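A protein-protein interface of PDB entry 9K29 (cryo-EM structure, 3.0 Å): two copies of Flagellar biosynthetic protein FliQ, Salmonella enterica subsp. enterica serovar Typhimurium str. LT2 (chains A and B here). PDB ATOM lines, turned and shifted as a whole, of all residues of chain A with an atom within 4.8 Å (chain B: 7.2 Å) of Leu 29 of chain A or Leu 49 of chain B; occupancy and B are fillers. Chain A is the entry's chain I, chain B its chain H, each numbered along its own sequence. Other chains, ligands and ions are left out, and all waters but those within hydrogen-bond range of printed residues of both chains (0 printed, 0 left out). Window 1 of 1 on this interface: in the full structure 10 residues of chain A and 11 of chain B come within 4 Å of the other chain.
Hydrophobic or aromatic side chains of chain A that line the printed part of chain B: Leu 25, Leu 29 and Leu 33. Along chain A the printed residues that touch a printed residue of chain B span positions 25 to 33. Of the 13 printed residues of chain B, 2 touch a printed residue of chain A. Hydrophobic or aromatic side chains of chain B that line the printed part of chain A: Leu 49 and Ile 52. Among the printed residues, 3 pairs touch across the chains. Among the printed residues, no Asp or Glu carboxylate lies within 4 Å of a Lys or Arg side-chain nitrogen of the other chain.
Printed residues of chain B within 4 Å of Leu 25 of chain A: Ile 52 (3.97 Å). Printed residues of chain A within 4 Å of Ile 52 of chain B: Leu 25 (3.97 Å). Thr 31 of chain A touches none of the printed residues of chain B. The nearest residue of chain A that does not touch Leu 49 of chain B is Gly 32 of chain A (4.5 Å). The nearest printed residue of chain B that does not touch Leu 25 of chain A is Phe 51 of chain B (4.4 Å).
Ile 52 of chain B touches Leu 25 of chain A. Leu 29 of chain A touches Leu 49 of chain B. Leu 33 of chain A touches Leu 49 of chain B.
No position is printed for both chains. Of the 3 pairs that touch across the chains among the printed residues, none has its exchanged pair printed and touching as well.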
ATOM      1  N   LEU A  25      -6.038 -10.357 -16.753  1.00  0.00           N
ATOM      2  CA  LEU A  25      -6.102 -10.900 -18.106  1.00  0.00           C
ATOM      3  C   LEU A  25      -6.597  -9.861 -19.103  1.00  0.00           C
ATOM      4  O   LEU A  25      -6.035  -9.731 -20.196  1.00  0.00           O
ATOM      5  CB  LEU A  25      -6.994 -12.141 -18.141  1.00  0.00           C
ATOM      6  CG  LEU A  25      -6.430 -13.407 -17.492  1.00  0.00           C
ATOM      7  CD1 LEU A  25      -7.554 -14.322 -17.036  1.00  0.00           C
ATOM      8  CD2 LEU A  25      -5.499 -14.131 -18.448  1.00  0.00           C
ATOM      9  N   LEU A  26      -7.646  -9.114 -18.753  1.00  0.00           N
ATOM     10  CA  LEU A  26      -8.171  -8.112 -19.679  1.00  0.00           C
ATOM     11  C   LEU A  26      -7.165  -6.992 -19.922  1.00  0.00           C
ATOM     12  O   LEU A  26      -6.994  -6.540 -21.059  1.00  0.00           O
ATOM     13  CB  LEU A  26      -9.504  -7.557 -19.176  1.00  0.00           C
ATOM     14  CG  LEU A  26     -10.774  -8.360 -19.493  1.00  0.00           C
ATOM     15  CD1 LEU A  26     -10.981  -8.392 -20.999  1.00  0.00           C
ATOM     16  CD2 LEU A  26     -10.760  -9.781 -18.944  1.00  0.00           C
ATOM     17  N   VAL A  27      -6.484  -6.529 -18.870  1.00  0.00           N
ATOM     18  CA  VAL A  27      -5.498  -5.470 -19.056  1.00  0.00           C
ATOM     19  C   VAL A  27      -4.330  -5.962 -19.902  1.00  0.00           C
ATOM     20  O   VAL A  27      -3.848  -5.247 -20.791  1.00  0.00           O
ATOM     21  CB  VAL A  27      -5.032  -4.921 -17.697  1.00  0.00           C
ATOM     22  CG1 VAL A  27      -3.925  -3.914 -17.891  1.00  0.00           C
ATOM     23  CG2 VAL A  27      -6.191  -4.253 -16.981  1.00  0.00           C
ATOM     24  N   ALA A  28      -3.858  -7.188 -19.654  1.00  0.00           N
ATOM     25  CA  ALA A  28      -2.771  -7.734 -20.459  1.00  0.00           C
ATOM     26  C   ALA A  28      -3.189  -7.883 -21.916  1.00  0.00           C
ATOM     27  O   ALA A  28      -2.423  -7.562 -22.831  1.00  0.00           O
ATOM     28  CB  ALA A  28      -2.317  -9.077 -19.886  1.00  0.00           C
ATOM     29  N   LEU A  29      -4.413  -8.362 -22.148  1.00  0.00           N
ATOM     30  CA  LEU A  29      -4.914  -8.512 -23.510  1.00  0.00           C
ATOM     31  C   LEU A  29      -5.001  -7.167 -24.217  1.00  0.00           C
ATOM     32  O   LEU A  29      -4.592  -7.040 -25.377  1.00  0.00           O
ATOM     33  CB  LEU A  29      -6.281  -9.194 -23.482  1.00  0.00           C
ATOM     34  CG  LEU A  29      -7.079  -9.269 -24.784  1.00  0.00           C
ATOM     35  CD1 LEU A  29      -6.417 -10.218 -25.760  1.00  0.00           C
ATOM     36  CD2 LEU A  29      -8.511  -9.695 -24.506  1.00  0.00           C
ATOM     37  N   ILE A  30      -5.523  -6.148 -23.530  1.00  0.00           N
ATOM     38  CA  ILE A  30      -5.664  -4.828 -24.137  1.00  0.00           C
ATOM     39  C   ILE A  30      -4.296  -4.243 -24.463  1.00  0.00           C
ATOM     40  O   ILE A  30      -4.080  -3.684 -25.545  1.00  0.00           O
ATOM     41  CB  ILE A  30      -6.473  -3.899 -23.215  1.00  0.00           C
ATOM     42  CG1 ILE A  30      -7.951  -4.288 -23.234  1.00  0.00           C
ATOM     43  CG2 ILE A  30      -6.298  -2.446 -23.626  1.00  0.00           C
ATOM     44  CD1 ILE A  30      -8.558  -4.311 -24.620  1.00  0.00           C
ATOM     45  N   THR A  31      -3.350  -4.360 -23.526  1.00  0.00           N
ATOM     46  CA  THR A  31      -2.013  -3.826 -23.761  1.00  0.00           C
ATOM     47  C   THR A  31      -1.335  -4.530 -24.929  1.00  0.00           C
ATOM     48  O   THR A  31      -0.741  -3.878 -25.796  1.00  0.00           O
ATOM     49  CB  THR A  31      -1.167  -3.952 -22.495  1.00  0.00           C
ATOM     50  OG1 THR A  31      -1.857  -3.339 -21.399  1.00  0.00           O
ATOM     51  CG2 THR A  31       0.176  -3.270 -22.685  1.00  0.00           C
ATOM     52  N   GLY A  32      -1.420  -5.861 -24.975  1.00  0.00           N
ATOM     53  CA  GLY A  32      -0.842  -6.584 -26.092  1.00  0.00           C
ATOM     54  C   GLY A  32      -1.472  -6.199 -27.416  1.00  0.00           C
ATOM     55  O   GLY A  32      -0.775  -6.005 -28.413  1.00  0.00           O
ATOM     56  N   LEU A  33      -2.801  -6.062 -27.436  1.00  0.00           N
ATOM     57  CA  LEU A  33      -3.493  -5.701 -28.667  1.00  0.00           C
ATOM     58  C   LEU A  33      -3.074  -4.320 -29.152  1.00  0.00           C
ATOM     59  O   LEU A  33      -2.799  -4.126 -30.342  1.00  0.00           O
ATOM     60  CB  LEU A  33      -5.005  -5.763 -28.450  1.00  0.00           C
ATOM     61  CG  LEU A  33      -5.879  -5.712 -29.702  1.00  0.00           C
ATOM     62  CD1 LEU A  33      -5.310  -6.602 -30.793  1.00  0.00           C
ATOM     63  CD2 LEU A  33      -7.307  -6.114 -29.370  1.00  0.00           C
ATOM     64  N   ILE B  35      -8.763 -16.859 -34.353  1.00  0.00           N
ATOM     65  CA  ILE B  35      -7.812 -15.816 -33.986  1.00  0.00           C
ATOM     66  C   ILE B  35      -6.599 -15.855 -34.908  1.00  0.00           C
ATOM     67  O   ILE B  35      -6.033 -14.813 -35.245  1.00  0.00           O
ATOM     68  CB  ILE B  35      -7.411 -15.938 -32.505  1.00  0.00           C
ATOM     69  CG1 ILE B  35      -8.640 -15.789 -31.610  1.00  0.00           C
ATOM     70  CG2 ILE B  35      -6.395 -14.871 -32.141  1.00  0.00           C
ATOM     71  CD1 ILE B  35      -9.351 -14.462 -31.768  1.00  0.00           C
ATOM     72  N   GLN B  39      -5.065 -12.922 -37.131  1.00  0.00           N
ATOM     73  CA  GLN B  39      -3.641 -12.602 -37.138  1.00  0.00           C
ATOM     74  C   GLN B  39      -3.050 -12.600 -38.540  1.00  0.00           C
ATOM     75  O   GLN B  39      -2.066 -11.893 -38.781  1.00  0.00           O
ATOM     76  CB  GLN B  39      -2.861 -13.600 -36.278  1.00  0.00           C
ATOM     77  CG  GLN B  39      -3.275 -13.662 -34.820  1.00  0.00           C
ATOM     78  CD  GLN B  39      -2.937 -12.404 -34.060  1.00  0.00           C
ATOM     79  OE1 GLN B  39      -1.867 -11.825 -34.237  1.00  0.00           O
ATOM     80  NE2 GLN B  39      -3.850 -11.973 -33.202  1.00  0.00           N
ATOM     81  N   ILE B  44      -0.725  -8.614 -37.632  1.00  0.00           N
ATOM     82  CA  ILE B  44      -0.536  -8.629 -36.187  1.00  0.00           C
ATOM     83  C   ILE B  44       0.313  -9.847 -35.855  1.00  0.00           C
ATOM     84  O   ILE B  44      -0.046 -10.978 -36.199  1.00  0.00           O
ATOM     85  CB  ILE B  44      -1.878  -8.660 -35.444  1.00  0.00           C
ATOM     86  CG1 ILE B  44      -2.760  -7.491 -35.886  1.00  0.00           C
ATOM     87  CG2 ILE B  44      -1.658  -8.624 -33.945  1.00  0.00           C
ATOM     88  CD1 ILE B  44      -2.157  -6.134 -35.607  1.00  0.00           C
ATOM     89  N   ASN B  45       1.449  -9.624 -35.195  1.00  0.00           N
ATOM     90  CA  ASN B  45       2.397 -10.688 -34.882  1.00  0.00           C
ATOM     91  C   ASN B  45       2.446 -11.009 -33.392  1.00  0.00           C
ATOM     92  O   ASN B  45       3.465 -11.504 -32.899  1.00  0.00           O
ATOM     93  CB  ASN B  45       3.796 -10.326 -35.387  1.00  0.00           C
ATOM     94  CG  ASN B  45       3.856 -10.144 -36.897  1.00  0.00           C
ATOM     95  OD1 ASN B  45       2.866 -10.369 -37.593  1.00  0.00           O
ATOM     96  ND2 ASN B  45       5.002  -9.707 -37.403  1.00  0.00           N
ATOM     97  N   GLU B  46       1.368 -10.736 -32.662  1.00  0.00           N
ATOM     98  CA  GLU B  46       1.331 -11.038 -31.238  1.00  0.00           C
ATOM     99  C   GLU B  46       1.207 -12.542 -31.030  1.00  0.00           C
ATOM    100  O   GLU B  46       0.394 -13.204 -31.681  1.00  0.00           O
ATOM    101  CB  GLU B  46       0.173 -10.310 -30.560  1.00  0.00           C
ATOM    102  CG  GLU B  46       0.096 -10.542 -29.060  1.00  0.00           C
ATOM    103  CD  GLU B  46       1.289  -9.975 -28.313  1.00  0.00           C
ATOM    104  OE1 GLU B  46       1.912  -9.016 -28.816  1.00  0.00           O
ATOM    105  OE2 GLU B  46       1.604 -10.491 -27.220  1.00  0.00           O
ATOM    106  N   MET B  47       2.018 -13.079 -30.117  1.00  0.00           N
ATOM    107  CA  MET B  47       2.088 -14.524 -29.934  1.00  0.00           C
ATOM    108  C   MET B  47       0.955 -15.039 -29.051  1.00  0.00           C
ATOM    109  O   MET B  47       0.204 -15.937 -29.449  1.00  0.00           O
ATOM    110  CB  MET B  47       3.449 -14.904 -29.346  1.00  0.00           C
ATOM    111  CG  MET B  47       3.656 -16.395 -29.160  1.00  0.00           C
ATOM    112  SD  MET B  47       5.287 -16.769 -28.493  1.00  0.00           S
ATOM    113  CE  MET B  47       5.101 -16.190 -26.810  1.00  0.00           C
ATOM    114  N   THR B  48       0.813 -14.480 -27.847  1.00  0.00           N
ATOM    115  CA  THR B  48      -0.154 -14.967 -26.871  1.00  0.00           C
ATOM    116  C   THR B  48      -1.472 -14.205 -26.909  1.00  0.00           C
ATOM    117  O   THR B  48      -2.168 -14.131 -25.888  1.00  0.00           O
ATOM    118  CB  THR B  48       0.440 -14.909 -25.463  1.00  0.00           C
ATOM    119  OG1 THR B  48       0.475 -13.549 -25.015  1.00  0.00           O
ATOM    120  CG2 THR B  48       1.845 -15.477 -25.457  1.00  0.00           C
ATOM    121  N   LEU B  49      -1.837 -13.632 -28.057  1.00  0.00           N
ATOM    122  CA  LEU B  49      -3.101 -12.909 -28.133  1.00  0.00           C
ATOM    123  C   LEU B  49      -4.285 -13.864 -28.182  1.00  0.00           C
ATOM    124  O   LEU B  49      -5.400 -13.488 -27.804  1.00  0.00           O
ATOM    125  CB  LEU B  49      -3.109 -11.985 -29.350  1.00  0.00           C
ATOM    126  CG  LEU B  49      -4.144 -10.861 -29.316  1.00  0.00           C
ATOM    127  CD1 LEU B  49      -3.815  -9.903 -28.187  1.00  0.00           C
ATOM    128  CD2 LEU B  49      -4.191 -10.119 -30.634  1.00  0.00           C
ATOM    129  N   SER B  50      -4.066 -15.097 -28.642  1.00  0.00           N
ATOM    130  CA  SER B  50      -5.146 -16.068 -28.757  1.00  0.00           C
ATOM    131  C   SER B  50      -5.425 -16.807 -27.456  1.00  0.00           C
ATOM    132  O   SER B  50      -6.447 -17.494 -27.361  1.00  0.00           O
ATOM    133  CB  SER B  50      -4.822 -17.088 -29.851  1.00  0.00           C
ATOM    134  OG  SER B  50      -4.060 -18.163 -29.333  1.00  0.00           O
ATOM    135  N   PHE B  51      -4.550 -16.684 -26.458  1.00  0.00           N
ATOM    136  CA  PHE B  51      -4.702 -17.470 -25.237  1.00  0.00           C
ATOM    137  C   PHE B  51      -5.971 -17.091 -24.481  1.00  0.00           C
ATOM    138  O   PHE B  51      -6.734 -17.964 -24.055  1.00  0.00           O
ATOM    139  CB  PHE B  51      -3.477 -17.297 -24.344  1.00  0.00           C
ATOM    140  CG  PHE B  51      -3.646 -17.883 -22.976  1.00  0.00           C
ATOM    141  CD1 PHE B  51      -3.655 -19.254 -22.793  1.00  0.00           C
ATOM    142  CD2 PHE B  51      -3.811 -17.064 -21.874  1.00  0.00           C
ATOM    143  CE1 PHE B  51      -3.814 -19.795 -21.535  1.00  0.00           C
ATOM    144  CE2 PHE B  51      -3.973 -17.598 -20.614  1.00  0.00           C
ATOM    145  CZ  PHE B  51      -3.976 -18.965 -20.445  1.00  0.00           C
ATOM    146  N   ILE B  52      -6.199 -15.790 -24.286  1.00  0.00           N
ATOM    147  CA  ILE B  52      -7.381 -15.350 -23.540  1.00  0.00           C
ATOM    148  C   ILE B  52      -8.680 -15.750 -24.231  1.00  0.00           C
ATOM    149  O   ILE B  52      -9.595 -16.233 -23.543  1.00  0.00           O
ATOM    150  CB  ILE B  52      -7.295 -13.838 -23.258  1.00  0.00           C
ATOM    151  CG1 ILE B  52      -6.123 -13.532 -22.323  1.00  0.00           C
ATOM    152  CG2 ILE B  52      -8.595 -13.331 -22.659  1.00  0.00           C
ATOM    153  CD1 ILE B  52      -4.850 -13.125 -23.038  1.00  0.00           C
ATOM    154  N   PRO B  53      -8.852 -15.559 -25.546  1.00  0.00           N
ATOM    155  CA  PRO B  53     -10.069 -16.079 -26.189  1.00  0.00           C
ATOM    156  C   PRO B  53     -10.227 -17.583 -26.059  1.00  0.00           C
ATOM    157  O   PRO B  53     -11.355 -18.063 -25.913  1.00  0.00           O
ATOM    158  CB  PRO B  53      -9.900 -15.654 -27.654  1.00  0.00           C
ATOM    159  CG  PRO B  53      -9.020 -14.466 -27.592  1.00  0.00           C
ATOM    160  CD  PRO B  53      -8.053 -14.755 -26.489  1.00  0.00           C
ATOM    161  N   LYS B  54      -9.130 -18.343 -26.103  1.00  0.00           N
ATOM    162  CA  LYS B  54      -9.231 -19.789 -25.921  1.00  0.00           C
ATOM    163  C   LYS B  54      -9.704 -20.134 -24.515  1.00  0.00           C
ATOM    164  O   LYS B  54     -10.542 -21.026 -24.333  1.00  0.00           O
ATOM    165  CB  LYS B  54      -7.885 -20.449 -26.215  1.00  0.00           C
ATOM    166  CG  LYS B  54      -7.506 -20.437 -27.683  1.00  0.00           C
ATOM    167  CD  LYS B  54      -6.081 -20.903 -27.888  1.00  0.00           C
ATOM    168  CE  LYS B  54      -5.951 -22.384 -27.609  1.00  0.00           C
ATOM    169  NZ  LYS B  54      -4.581 -22.876 -27.902  1.00  0.00           N
